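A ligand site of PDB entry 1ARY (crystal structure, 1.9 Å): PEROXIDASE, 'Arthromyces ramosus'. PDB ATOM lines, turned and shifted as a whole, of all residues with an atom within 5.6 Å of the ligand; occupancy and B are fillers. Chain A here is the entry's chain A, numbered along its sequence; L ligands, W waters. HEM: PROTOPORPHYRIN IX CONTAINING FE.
The side-chain hydroxyl (OG) of Ser 245 sits at hydrogen-bond distance from the side-chain sulfur (SD) of Met 243 (3.4 Å).
OE1 of Gln 189 sits at hydrogen-bond distance from N of Leu 192 (3.1 Å).
O of Pro 156 lies within hydrogen-bond range of N of Ser 245 (3.3 Å).
The backbone NH (N) of Leu 201 sits at hydrogen-bond distance from the backbone carbonyl oxygen (O) of Ala 187, 3.0 Å away.
The side-chain carboxylate (OE1) of Glu 190 is in salt-bridge range of the side-chain amino group (NZ) of Lys 49.
Lys 49 touches the ligand (CD to O1D, 3.8 Å).
O of Leu 51 touches CAC of the ligand (3.4 Å).
Phe 55 touches the ligand.
Pro 154 touches the ligand (O to CMB, 3.9 Å).
Gly 155 touches the ligand.
Pro 156 touches the ligand (CG to CMA, 3.6 Å).
Ile 163 touches the ligand.
Leu 180 touches the ligand (CB to CMC, 3.9 Å).
CD2 of Leu 181 touches CHC of the ligand, 3.7 Å away.
Ala 183 touches the ligand.
O of Leu 186 touches CMD of the ligand, at 3.5 Å.
Ala 187 touches the ligand (CB to CAD, 3.4 Å).
CA of Gln 189 touches O1A of the ligand, 3.6 Å away.
Leu 192 touches the ligand.
Met 243 touches the ligand.
Ser 245 touches the ligand (OG to CMB, 3.7 Å).
Met 277 touches the ligand (SD to CBC, 3.9 Å).
Of the 32 residues printed, 23 come within 4 Å of the ligand.
Along chain A the residues within 4 Å of the ligand span positions 48 to 277.
The nearest printed residue that does not touch the ligand is Tyr 273 (4.1 Å).
The backbone NH (N) of Glu 190 sits at hydrogen-bond distance from an oxygen (O1A) of the ligand, 2.8 Å away.
The side-chain hydroxyl (OG) of Ser 188 is in hydrogen-bond range of an oxygen (O2D) of the ligand (2.9 Å).
A ring nitrogen (NE2) of His 184 is bound to an iron atom (FE) of the ligand (2.1 Å).
An oxygen (O2D) of the ligand lies within salt-bridge range of the guanidinium group of Arg 48, 2.9 Å away.
An oxygen (O1A) of the ligand lies within salt-bridge range of the guanidinium group (NH1) of Arg 52 (3.99 Å).
The backbone NH (N) of Ser 188 sits at hydrogen-bond distance from an oxygen (O2D) of the ligand, at 2.9 Å.
N of Gly 191 lies within hydrogen-bond range of O2A of the ligand (3.0 Å).
Water W2 lies within hydrogen-bond range of O1D of the ligand (2.6 Å), OE2 of Glu 190 (2.8 Å), OG of Ser 45 (2.8 Å) and NH2 of Arg 48 (3.0 Å).
Water W1 lies within hydrogen-bond range of O1A of the ligand (2.7 Å), NZ of Lys 49 (2.8 Å) and NH1 of Arg 52 (2.9 Å).
Water W4 lies within hydrogen-bond range of O1A of the ligand (3.0 Å) and NH1 of Arg 52 (3.2 Å).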
ATOM      1  N   SER A  45     -28.472  30.542  -6.648  1.00  0.00           N
ATOM      2  CA  SER A  45     -27.469  29.775  -5.956  1.00  0.00           C
ATOM      3  C   SER A  45     -27.673  29.553  -4.452  1.00  0.00           C
ATOM      4  O   SER A  45     -27.474  28.398  -4.059  1.00  0.00           O
ATOM      5  CB  SER A  45     -26.126  30.441  -6.243  1.00  0.00           C
ATOM      6  OG  SER A  45     -25.053  29.674  -5.685  1.00  0.00           O
ATOM      7  N   VAL A  47     -30.303  28.971  -2.659  1.00  0.00           N
ATOM      8  CA  VAL A  47     -31.260  27.853  -2.537  1.00  0.00           C
ATOM      9  C   VAL A  47     -30.570  26.525  -2.931  1.00  0.00           C
ATOM     10  O   VAL A  47     -30.657  25.517  -2.220  1.00  0.00           O
ATOM     11  CB  VAL A  47     -32.491  28.091  -3.472  1.00  0.00           C
ATOM     12  CG1 VAL A  47     -33.475  26.956  -3.284  1.00  0.00           C
ATOM     13  CG2 VAL A  47     -33.200  29.388  -3.152  1.00  0.00           C
ATOM     14  N   ARG A  48     -29.857  26.476  -4.059  1.00  0.00           N
ATOM     15  CA  ARG A  48     -29.157  25.265  -4.522  1.00  0.00           C
ATOM     16  C   ARG A  48     -28.102  24.822  -3.526  1.00  0.00           C
ATOM     17  O   ARG A  48     -27.990  23.631  -3.236  1.00  0.00           O
ATOM     18  CB  ARG A  48     -28.500  25.522  -5.896  1.00  0.00           C
ATOM     19  CG  ARG A  48     -29.506  25.964  -6.933  1.00  0.00           C
ATOM     20  CD  ARG A  48     -28.988  25.893  -8.340  1.00  0.00           C
ATOM     21  NE  ARG A  48     -27.754  26.649  -8.544  1.00  0.00           N
ATOM     22  CZ  ARG A  48     -27.774  27.870  -9.037  1.00  0.00           C
ATOM     23  NH1 ARG A  48     -28.900  28.485  -9.384  1.00  0.00           N
ATOM     24  NH2 ARG A  48     -26.601  28.454  -9.272  1.00  0.00           N
ATOM     25  N   LYS A  49     -27.369  25.739  -2.919  1.00  0.00           N
ATOM     26  CA  LYS A  49     -26.393  25.413  -1.899  1.00  0.00           C
ATOM     27  C   LYS A  49     -27.077  24.897  -0.649  1.00  0.00           C
ATOM     28  O   LYS A  49     -26.633  23.914  -0.063  1.00  0.00           O
ATOM     29  CB  LYS A  49     -25.572  26.657  -1.514  1.00  0.00           C
ATOM     30  CG  LYS A  49     -24.729  27.296  -2.621  1.00  0.00           C
ATOM     31  CD  LYS A  49     -23.655  26.319  -3.072  1.00  0.00           C
ATOM     32  CE  LYS A  49     -22.675  27.024  -3.990  1.00  0.00           C
ATOM     33  NZ  LYS A  49     -21.530  26.181  -4.258  1.00  0.00           N
ATOM     34  N   LEU A  51     -29.812  23.274  -0.469  1.00  0.00           N
ATOM     35  CA  LEU A  51     -30.297  21.935  -0.753  1.00  0.00           C
ATOM     36  C   LEU A  51     -29.178  20.903  -0.616  1.00  0.00           C
ATOM     37  O   LEU A  51     -29.430  19.783  -0.153  1.00  0.00           O
ATOM     38  CB  LEU A  51     -30.919  21.903  -2.145  1.00  0.00           C
ATOM     39  CG  LEU A  51     -32.358  22.404  -2.214  1.00  0.00           C
ATOM     40  CD1 LEU A  51     -32.825  22.585  -3.628  1.00  0.00           C
ATOM     41  CD2 LEU A  51     -33.241  21.378  -1.499  1.00  0.00           C
ATOM     42  N   ARG A  52     -27.934  21.247  -0.969  1.00  0.00           N
ATOM     43  CA  ARG A  52     -26.789  20.353  -0.732  1.00  0.00           C
ATOM     44  C   ARG A  52     -26.553  20.223   0.775  1.00  0.00           C
ATOM     45  O   ARG A  52     -26.348  19.129   1.288  1.00  0.00           O
ATOM     46  CB  ARG A  52     -25.487  20.887  -1.367  1.00  0.00           C
ATOM     47  CG  ARG A  52     -25.391  20.715  -2.869  1.00  0.00           C
ATOM     48  CD  ARG A  52     -24.088  21.220  -3.436  1.00  0.00           C
ATOM     49  NE  ARG A  52     -22.970  20.469  -2.903  1.00  0.00           N
ATOM     50  CZ  ARG A  52     -21.737  20.998  -2.807  1.00  0.00           C
ATOM     51  NH1 ARG A  52     -21.442  22.240  -3.196  1.00  0.00           N
ATOM     52  NH2 ARG A  52     -20.771  20.260  -2.265  1.00  0.00           N
ATOM     53  N   VAL A  54     -28.711  20.519   3.445  1.00  0.00           N
ATOM     54  CA  VAL A  54     -29.721  19.764   4.191  1.00  0.00           C
ATOM     55  C   VAL A  54     -29.438  18.257   4.029  1.00  0.00           C
ATOM     56  O   VAL A  54     -29.380  17.530   5.022  1.00  0.00           O
ATOM     57  CB  VAL A  54     -31.124  20.234   3.645  1.00  0.00           C
ATOM     58  CG1 VAL A  54     -31.448  19.703   2.274  1.00  0.00           C
ATOM     59  CG2 VAL A  54     -32.176  19.782   4.639  1.00  0.00           C
ATOM     60  N   PHE A  55     -29.102  17.819   2.813  1.00  0.00           N
ATOM     61  CA  PHE A  55     -28.747  16.449   2.515  1.00  0.00           C
ATOM     62  C   PHE A  55     -27.470  16.102   3.249  1.00  0.00           C
ATOM     63  O   PHE A  55     -27.463  15.109   3.986  1.00  0.00           O
ATOM     64  CB  PHE A  55     -28.527  16.256   1.006  1.00  0.00           C
ATOM     65  CG  PHE A  55     -28.098  14.831   0.597  1.00  0.00           C
ATOM     66  CD1 PHE A  55     -28.657  13.706   1.178  1.00  0.00           C
ATOM     67  CD2 PHE A  55     -27.129  14.676  -0.365  1.00  0.00           C
ATOM     68  CE1 PHE A  55     -28.230  12.441   0.803  1.00  0.00           C
ATOM     69  CE2 PHE A  55     -26.711  13.416  -0.741  1.00  0.00           C
ATOM     70  CZ  PHE A  55     -27.248  12.293  -0.151  1.00  0.00           C
ATOM     71  N   PRO A 154     -22.517   9.858  -0.119  1.00  0.00           N
ATOM     72  CA  PRO A 154     -22.443   9.318  -1.472  1.00  0.00           C
ATOM     73  C   PRO A 154     -21.749  10.326  -2.386  1.00  0.00           C
ATOM     74  O   PRO A 154     -22.041  11.524  -2.326  1.00  0.00           O
ATOM     75  CB  PRO A 154     -23.890   9.079  -1.890  1.00  0.00           C
ATOM     76  CG  PRO A 154     -24.653   9.021  -0.593  1.00  0.00           C
ATOM     77  CD  PRO A 154     -23.911  10.013   0.294  1.00  0.00           C
ATOM     78  N   GLY A 155     -20.837   9.881  -3.238  1.00  0.00           N
ATOM     79  CA  GLY A 155     -20.167  10.776  -4.145  1.00  0.00           C
ATOM     80  C   GLY A 155     -20.578  10.485  -5.572  1.00  0.00           C
ATOM     81  O   GLY A 155     -21.110   9.408  -5.876  1.00  0.00           O
ATOM     82  N   PRO A 156     -20.315  11.394  -6.498  1.00  0.00           N
ATOM     83  CA  PRO A 156     -20.630  11.231  -7.905  1.00  0.00           C
ATOM     84  C   PRO A 156     -19.896  10.119  -8.649  1.00  0.00           C
ATOM     85  O   PRO A 156     -20.386   9.683  -9.701  1.00  0.00           O
ATOM     86  CB  PRO A 156     -20.407  12.607  -8.469  1.00  0.00           C
ATOM     87  CG  PRO A 156     -19.292  13.148  -7.624  1.00  0.00           C
ATOM     88  CD  PRO A 156     -19.750  12.710  -6.230  1.00  0.00           C
ATOM     89  N   ILE A 163     -24.100   3.535  -3.601  1.00  0.00           N
ATOM     90  CA  ILE A 163     -25.058   4.569  -3.237  1.00  0.00           C
ATOM     91  C   ILE A 163     -26.254   3.945  -2.551  1.00  0.00           C
ATOM     92  O   ILE A 163     -26.552   4.311  -1.401  1.00  0.00           O
ATOM     93  CB  ILE A 163     -25.476   5.352  -4.496  1.00  0.00           C
ATOM     94  CG1 ILE A 163     -24.275   6.165  -4.969  1.00  0.00           C
ATOM     95  CG2 ILE A 163     -26.659   6.277  -4.216  1.00  0.00           C
ATOM     96  CD1 ILE A 163     -24.412   6.906  -6.314  1.00  0.00           C
ATOM     97  N   MET A 167     -27.343   4.795   1.352  1.00  0.00           N
ATOM     98  CA  MET A 167     -28.675   5.373   1.499  1.00  0.00           C
ATOM     99  C   MET A 167     -29.621   4.398   2.193  1.00  0.00           C
ATOM    100  O   MET A 167     -30.444   4.833   3.005  1.00  0.00           O
ATOM    101  CB  MET A 167     -29.220   5.744   0.124  1.00  0.00           C
ATOM    102  CG  MET A 167     -28.460   6.889  -0.557  1.00  0.00           C
ATOM    103  SD  MET A 167     -28.551   8.444   0.362  1.00  0.00           S
ATOM    104  CE  MET A 167     -30.189   9.013  -0.049  1.00  0.00           C
ATOM    105  N   VAL A 177     -34.497   7.023  -2.999  1.00  0.00           N
ATOM    106  CA  VAL A 177     -33.246   7.596  -3.489  1.00  0.00           C
ATOM    107  C   VAL A 177     -33.588   8.347  -4.762  1.00  0.00           C
ATOM    108  O   VAL A 177     -33.278   9.540  -4.893  1.00  0.00           O
ATOM    109  CB  VAL A 177     -32.203   6.477  -3.783  1.00  0.00           C
ATOM    110  CG1 VAL A 177     -30.928   7.018  -4.450  1.00  0.00           C
ATOM    111  CG2 VAL A 177     -31.819   5.848  -2.437  1.00  0.00           C
ATOM    112  N   LEU A 180     -35.591  11.518  -3.922  1.00  0.00           N
ATOM    113  CA  LEU A 180     -34.762  12.572  -3.349  1.00  0.00           C
ATOM    114  C   LEU A 180     -34.006  13.355  -4.437  1.00  0.00           C
ATOM    115  O   LEU A 180     -33.819  14.578  -4.327  1.00  0.00           O
ATOM    116  CB  LEU A 180     -33.782  11.927  -2.397  1.00  0.00           C
ATOM    117  CG  LEU A 180     -33.774  12.145  -0.908  1.00  0.00           C
ATOM    118  CD1 LEU A 180     -34.990  12.874  -0.407  1.00  0.00           C
ATOM    119  CD2 LEU A 180     -33.581  10.781  -0.291  1.00  0.00           C
ATOM    120  N   LEU A 181     -33.618  12.669  -5.513  1.00  0.00           N
ATOM    121  CA  LEU A 181     -32.868  13.286  -6.583  1.00  0.00           C
ATOM    122  C   LEU A 181     -33.678  14.249  -7.426  1.00  0.00           C
ATOM    123  O   LEU A 181     -33.165  14.794  -8.404  1.00  0.00           O
ATOM    124  CB  LEU A 181     -32.247  12.235  -7.463  1.00  0.00           C
ATOM    125  CG  LEU A 181     -31.037  11.579  -6.819  1.00  0.00           C
ATOM    126  CD1 LEU A 181     -30.712  10.326  -7.555  1.00  0.00           C
ATOM    127  CD2 LEU A 181     -29.831  12.492  -6.865  1.00  0.00           C
ATOM    128  N   ALA A 183     -34.312  17.002  -6.424  1.00  0.00           N
ATOM    129  CA  ALA A 183     -33.648  18.276  -6.116  1.00  0.00           C
ATOM    130  C   ALA A 183     -32.620  18.662  -7.196  1.00  0.00           C
ATOM    131  O   ALA A 183     -32.274  19.832  -7.343  1.00  0.00           O
ATOM    132  CB  ALA A 183     -32.921  18.214  -4.785  1.00  0.00           C
ATOM    133  N   HIS A 184     -32.193  17.741  -8.063  1.00  0.00           N
ATOM    134  CA  HIS A 184     -31.254  18.085  -9.132  1.00  0.00           C
ATOM    135  C   HIS A 184     -31.989  18.794 -10.287  1.00  0.00           C
ATOM    136  O   HIS A 184     -31.435  19.187 -11.321  1.00  0.00           O
ATOM    137  CB  HIS A 184     -30.551  16.823  -9.655  1.00  0.00           C
ATOM    138  CG  HIS A 184     -29.360  16.326  -8.823  1.00  0.00           C
ATOM    139  ND1 HIS A 184     -28.487  15.339  -9.228  1.00  0.00           N
ATOM    140  CD2 HIS A 184     -28.975  16.837  -7.592  1.00  0.00           C
ATOM    141  CE1 HIS A 184     -27.558  15.268  -8.257  1.00  0.00           C
ATOM    142  NE2 HIS A 184     -27.810  16.108  -7.301  1.00  0.00           N
ATOM    143  N   LEU A 186     -33.158  21.640  -9.731  1.00  0.00           N
ATOM    144  CA  LEU A 186     -32.846  23.024  -9.403  1.00  0.00           C
ATOM    145  C   LEU A 186     -31.342  22.925  -9.111  1.00  0.00           C
ATOM    146  O   LEU A 186     -30.935  23.147  -7.977  1.00  0.00           O
ATOM    147  CB  LEU A 186     -33.634  23.422  -8.141  1.00  0.00           C
ATOM    148  CG  LEU A 186     -34.923  24.288  -8.001  1.00  0.00           C
ATOM    149  CD1 LEU A 186     -35.644  24.459  -9.296  1.00  0.00           C
ATOM    150  CD2 LEU A 186     -35.808  23.620  -6.959  1.00  0.00           C
ATOM    151  N   ALA A 187     -30.492  22.625 -10.068  1.00  0.00           N
ATOM    152  CA  ALA A 187     -29.092  22.368  -9.748  1.00  0.00           C
ATOM    153  C   ALA A 187     -28.079  22.659 -10.826  1.00  0.00           C
ATOM    154  O   ALA A 187     -28.372  22.648 -12.032  1.00  0.00           O
ATOM    155  CB  ALA A 187     -28.916  20.914  -9.397  1.00  0.00           C
ATOM    156  N   SER A 188     -26.855  22.862 -10.375  1.00  0.00           N
ATOM    157  CA  SER A 188     -25.761  23.074 -11.312  1.00  0.00           C
ATOM    158  C   SER A 188     -24.546  22.486 -10.613  1.00  0.00           C
ATOM    159  O   SER A 188     -24.672  21.955  -9.500  1.00  0.00           O
ATOM    160  CB  SER A 188     -25.546  24.570 -11.544  1.00  0.00           C
ATOM    161  OG  SER A 188     -24.977  25.285 -10.456  1.00  0.00           O
ATOM    162  N   GLN A 189     -23.397  22.535 -11.245  1.00  0.00           N
ATOM    163  CA  GLN A 189     -22.198  22.091 -10.560  1.00  0.00           C
ATOM    164  C   GLN A 189     -21.212  23.263 -10.591  1.00  0.00           C
ATOM    165  O   GLN A 189     -21.206  24.057 -11.549  1.00  0.00           O
ATOM    166  CB  GLN A 189     -21.621  20.849 -11.281  1.00  0.00           C
ATOM    167  CG  GLN A 189     -21.207  21.073 -12.746  1.00  0.00           C
ATOM    168  CD  GLN A 189     -19.793  21.611 -12.932  1.00  0.00           C
ATOM    169  OE1 GLN A 189     -18.932  21.474 -12.048  1.00  0.00           O
ATOM    170  NE2 GLN A 189     -19.492  22.196 -14.060  1.00  0.00           N
ATOM    171  N   GLU A 190     -20.338  23.374  -9.611  1.00  0.00           N
ATOM    172  CA  GLU A 190     -19.304  24.404  -9.600  1.00  0.00           C
ATOM    173  C   GLU A 190     -17.893  23.818  -9.469  1.00  0.00           C
ATOM    174  O   GLU A 190     -16.938  24.370 -10.022  1.00  0.00           O
ATOM    175  CB  GLU A 190     -19.496  25.363  -8.447  1.00  0.00           C
ATOM    176  CG  GLU A 190     -20.737  26.244  -8.567  1.00  0.00           C
ATOM    177  CD  GLU A 190     -20.946  27.234  -7.421  1.00  0.00           C
ATOM    178  OE1 GLU A 190     -20.163  27.243  -6.488  1.00  0.00           O
ATOM    179  OE2 GLU A 190     -21.911  27.997  -7.425  1.00  0.00           O
ATOM    180  N   GLY A 191     -17.763  22.683  -8.761  1.00  0.00           N
ATOM    181  CA  GLY A 191     -16.481  22.030  -8.469  1.00  0.00           C
ATOM    182  C   GLY A 191     -16.106  20.778  -9.237  1.00  0.00           C
ATOM    183  O   GLY A 191     -14.989  20.283  -9.083  1.00  0.00           O
ATOM    184  N   LEU A 192     -16.940  20.195 -10.075  1.00  0.00           N
ATOM    185  CA  LEU A 192     -16.579  19.009 -10.838  1.00  0.00           C
ATOM    186  C   LEU A 192     -15.870  19.412 -12.113  1.00  0.00           C
ATOM    187  O   LEU A 192     -14.993  18.703 -12.604  1.00  0.00           O
ATOM    188  CB  LEU A 192     -17.853  18.245 -11.135  1.00  0.00           C
ATOM    189  CG  LEU A 192     -18.291  17.008 -10.324  1.00  0.00           C
ATOM    190  CD1 LEU A 192     -17.967  17.115  -8.843  1.00  0.00           C
ATOM    191  CD2 LEU A 192     -19.754  16.831 -10.614  1.00  0.00           C
ATOM    192  N   LEU A 201     -27.870  21.053 -14.467  1.00  0.00           N
ATOM    193  CA  LEU A 201     -28.105  19.642 -14.594  1.00  0.00           C
ATOM    194  C   LEU A 201     -29.385  19.431 -15.391  1.00  0.00           C
ATOM    195  O   LEU A 201     -29.597  18.319 -15.907  1.00  0.00           O
ATOM    196  CB  LEU A 201     -28.117  19.068 -13.174  1.00  0.00           C
ATOM    197  CG  LEU A 201     -26.805  18.429 -12.567  1.00  0.00           C
ATOM    198  CD1 LEU A 201     -25.545  19.188 -12.895  1.00  0.00           C
ATOM    199  CD2 LEU A 201     -27.020  18.338 -11.073  1.00  0.00           C
ATOM    200  N   MET A 243     -23.614  14.211 -14.520  1.00  0.00           N
ATOM    201  CA  MET A 243     -22.672  13.483 -13.702  1.00  0.00           C
ATOM    202  C   MET A 243     -22.997  11.972 -13.773  1.00  0.00           C
ATOM    203  O   MET A 243     -24.128  11.509 -13.999  1.00  0.00           O
ATOM    204  CB  MET A 243     -22.723  13.984 -12.227  1.00  0.00           C
ATOM    205  CG  MET A 243     -23.968  13.619 -11.437  1.00  0.00           C
ATOM    206  SD  MET A 243     -24.007  14.235  -9.743  1.00  0.00           S
ATOM    207  CE  MET A 243     -24.586  15.838 -10.257  1.00  0.00           C
ATOM    208  N   SER A 245     -23.161   9.431 -11.446  1.00  0.00           N
ATOM    209  CA  SER A 245     -24.118   8.810 -10.558  1.00  0.00           C
ATOM    210  C   SER A 245     -25.539   8.960 -11.079  1.00  0.00           C
ATOM    211  O   SER A 245     -26.311   8.008 -11.061  1.00  0.00           O
ATOM    212  CB  SER A 245     -23.972   9.435  -9.186  1.00  0.00           C
ATOM    213  OG  SER A 245     -24.034  10.853  -9.294  1.00  0.00           O
ATOM    214  N   LEU A 249     -27.909   5.787 -12.346  1.00  0.00           N
ATOM    215  CA  LEU A 249     -29.163   5.548 -11.627  1.00  0.00           C
ATOM    216  C   LEU A 249     -30.370   5.569 -12.551  1.00  0.00           C
ATOM    217  O   LEU A 249     -31.309   4.788 -12.376  1.00  0.00           O
ATOM    218  CB  LEU A 249     -29.326   6.596 -10.526  1.00  0.00           C
ATOM    219  CG  LEU A 249     -28.498   6.412  -9.239  1.00  0.00           C
ATOM    220  CD1 LEU A 249     -28.501   7.692  -8.452  1.00  0.00           C
ATOM    221  CD2 LEU A 249     -29.074   5.264  -8.406  1.00  0.00           C
ATOM    222  N   TYR A 273     -41.246  13.583  -3.671  1.00  0.00           N
ATOM    223  CA  TYR A 273     -40.126  14.343  -3.104  1.00  0.00           C
ATOM    224  C   TYR A 273     -40.477  14.856  -1.710  1.00  0.00           C
ATOM    225  O   TYR A 273     -39.684  14.684  -0.785  1.00  0.00           O
ATOM    226  CB  TYR A 273     -39.792  15.529  -4.025  1.00  0.00           C
ATOM    227  CG  TYR A 273     -38.689  16.460  -3.549  1.00  0.00           C
ATOM    228  CD1 TYR A 273     -37.366  16.056  -3.624  1.00  0.00           C
ATOM    229  CD2 TYR A 273     -39.025  17.725  -3.073  1.00  0.00           C
ATOM    230  CE1 TYR A 273     -36.367  16.916  -3.244  1.00  0.00           C
ATOM    231  CE2 TYR A 273     -38.022  18.594  -2.694  1.00  0.00           C
ATOM    232  CZ  TYR A 273     -36.704  18.174  -2.796  1.00  0.00           C
ATOM    233  OH  TYR A 273     -35.710  19.042  -2.438  1.00  0.00           O
ATOM    234  N   MET A 277     -38.315  14.034   1.570  1.00  0.00           N
ATOM    235  CA  MET A 277     -37.703  15.083   2.363  1.00  0.00           C
ATOM    236  C   MET A 277     -38.209  15.093   3.785  1.00  0.00           C
ATOM    237  O   MET A 277     -37.419  15.338   4.704  1.00  0.00           O
ATOM    238  CB  MET A 277     -37.963  16.457   1.786  1.00  0.00           C
ATOM    239  CG  MET A 277     -37.226  16.661   0.464  1.00  0.00           C
ATOM    240  SD  MET A 277     -35.426  16.657   0.648  1.00  0.00           S
ATOM    241  CE  MET A 277     -35.291  18.248   1.402  1.00  0.00           C
ATOM    242  N   MET A 280     -36.170  12.436   5.568  1.00  0.00           N
ATOM    243  CA  MET A 280     -34.807  12.887   5.773  1.00  0.00           C
ATOM    244  C   MET A 280     -34.711  13.935   6.871  1.00  0.00           C
ATOM    245  O   MET A 280     -33.724  13.931   7.620  1.00  0.00           O
ATOM    246  CB  MET A 280     -34.274  13.469   4.468  1.00  0.00           C
ATOM    247  CG  MET A 280     -32.781  13.730   4.553  1.00  0.00           C
ATOM    248  SD  MET A 280     -31.960  14.026   2.983  1.00  0.00           S
ATOM    249  CE  MET A 280     -32.395  15.732   2.771  1.00  0.00           C
HETATM  250  CHA HEM L   1     -25.282  19.247  -6.829  1.00  0.00           C
HETATM  251  CHB HEM L   1     -24.000  14.660  -6.206  1.00  0.00           C
HETATM  252  CHC HEM L   1     -28.108  13.838  -3.905  1.00  0.00           C
HETATM  253  CHD HEM L   1     -29.140  18.474  -4.112  1.00  0.00           C
HETATM  254  C1A HEM L   1     -24.560  18.056  -6.876  1.00  0.00           C
HETATM  255  C2A HEM L   1     -23.197  17.941  -7.339  1.00  0.00           C
HETATM  256  C3A HEM L   1     -22.837  16.662  -7.154  1.00  0.00           C
HETATM  257  C4A HEM L   1     -23.958  15.989  -6.550  1.00  0.00           C
HETATM  258  CMA HEM L   1     -21.511  16.044  -7.529  1.00  0.00           C
HETATM  259  CAA HEM L   1     -22.333  19.087  -7.836  1.00  0.00           C
HETATM  260  CBA HEM L   1     -21.734  19.894  -6.687  1.00  0.00           C
HETATM  261  CGA HEM L   1     -20.781  20.969  -7.189  1.00  0.00           C
HETATM  262  O1A HEM L   1     -21.118  22.158  -7.167  1.00  0.00           O
HETATM  263  O2A HEM L   1     -19.685  20.641  -7.629  1.00  0.00           O
HETATM  264  C1B HEM L   1     -25.072  14.011  -5.638  1.00  0.00           C
HETATM  265  C2B HEM L   1     -25.129  12.568  -5.369  1.00  0.00           C
HETATM  266  C3B HEM L   1     -26.320  12.323  -4.731  1.00  0.00           C
HETATM  267  C4B HEM L   1     -26.969  13.627  -4.630  1.00  0.00           C
HETATM  268  CMB HEM L   1     -24.041  11.555  -5.699  1.00  0.00           C
HETATM  269  CAB HEM L   1     -26.801  11.126  -4.176  1.00  0.00           C
HETATM  270  CBB HEM L   1     -27.177   9.933  -4.907  1.00  0.00           C
HETATM  271  C1C HEM L   1     -28.703  15.042  -3.719  1.00  0.00           C
HETATM  272  C2C HEM L   1     -29.793  15.235  -2.816  1.00  0.00           C
HETATM  273  C3C HEM L   1     -30.034  16.576  -2.770  1.00  0.00           C
HETATM  274  C4C HEM L   1     -29.118  17.168  -3.723  1.00  0.00           C
HETATM  275  CMC HEM L   1     -30.526  14.102  -2.119  1.00  0.00           C
HETATM  276  CAC HEM L   1     -30.880  17.306  -1.935  1.00  0.00           C
HETATM  277  CBC HEM L   1     -32.235  16.982  -1.503  1.00  0.00           C
HETATM  278  C1D HEM L   1     -28.269  19.059  -5.001  1.00  0.00           C
HETATM  279  C2D HEM L   1     -28.348  20.440  -5.439  1.00  0.00           C
HETATM  280  C3D HEM L   1     -27.239  20.662  -6.163  1.00  0.00           C
HETATM  281  C4D HEM L   1     -26.517  19.425  -6.209  1.00  0.00           C
HETATM  282  CMD HEM L   1     -29.528  21.392  -5.279  1.00  0.00           C
HETATM  283  CAD HEM L   1     -26.874  21.956  -6.853  1.00  0.00           C
HETATM  284  CBD HEM L   1     -25.903  22.858  -6.122  1.00  0.00           C
HETATM  285  CGD HEM L   1     -25.571  24.141  -6.881  1.00  0.00           C
HETATM  286  O1D HEM L   1     -24.791  24.927  -6.377  1.00  0.00           O
HETATM  287  O2D HEM L   1     -26.079  24.377  -7.968  1.00  0.00           O
HETATM  288  NA  HEM L   1     -25.001  16.863  -6.363  1.00  0.00           N
HETATM  289  NB  HEM L   1     -26.227  14.640  -5.228  1.00  0.00           N
HETATM  290  NC  HEM L   1     -28.272  16.230  -4.272  1.00  0.00           N
HETATM  291  ND  HEM L   1     -27.200  18.429  -5.554  1.00  0.00           N
HETATM  292 FE   HEM L   1     -26.755  16.527  -5.512  1.00  0.00          FE
HETATM  293  O   HOH W   1     -22.450  23.765  -5.444  1.00  0.00           O
HETATM  294  O   HOH W   2     -24.620  27.395  -7.321  1.00  0.00           O
HETATM  295  O   HOH W   3     -26.553  11.352  -8.096  1.00  0.00           O
HETATM  296  O   HOH W   4     -19.280  23.441  -5.171  1.00  0.00           O
HETATM  297  O   HOH W   5     -17.835  19.119  -6.204  1.00  0.00           O
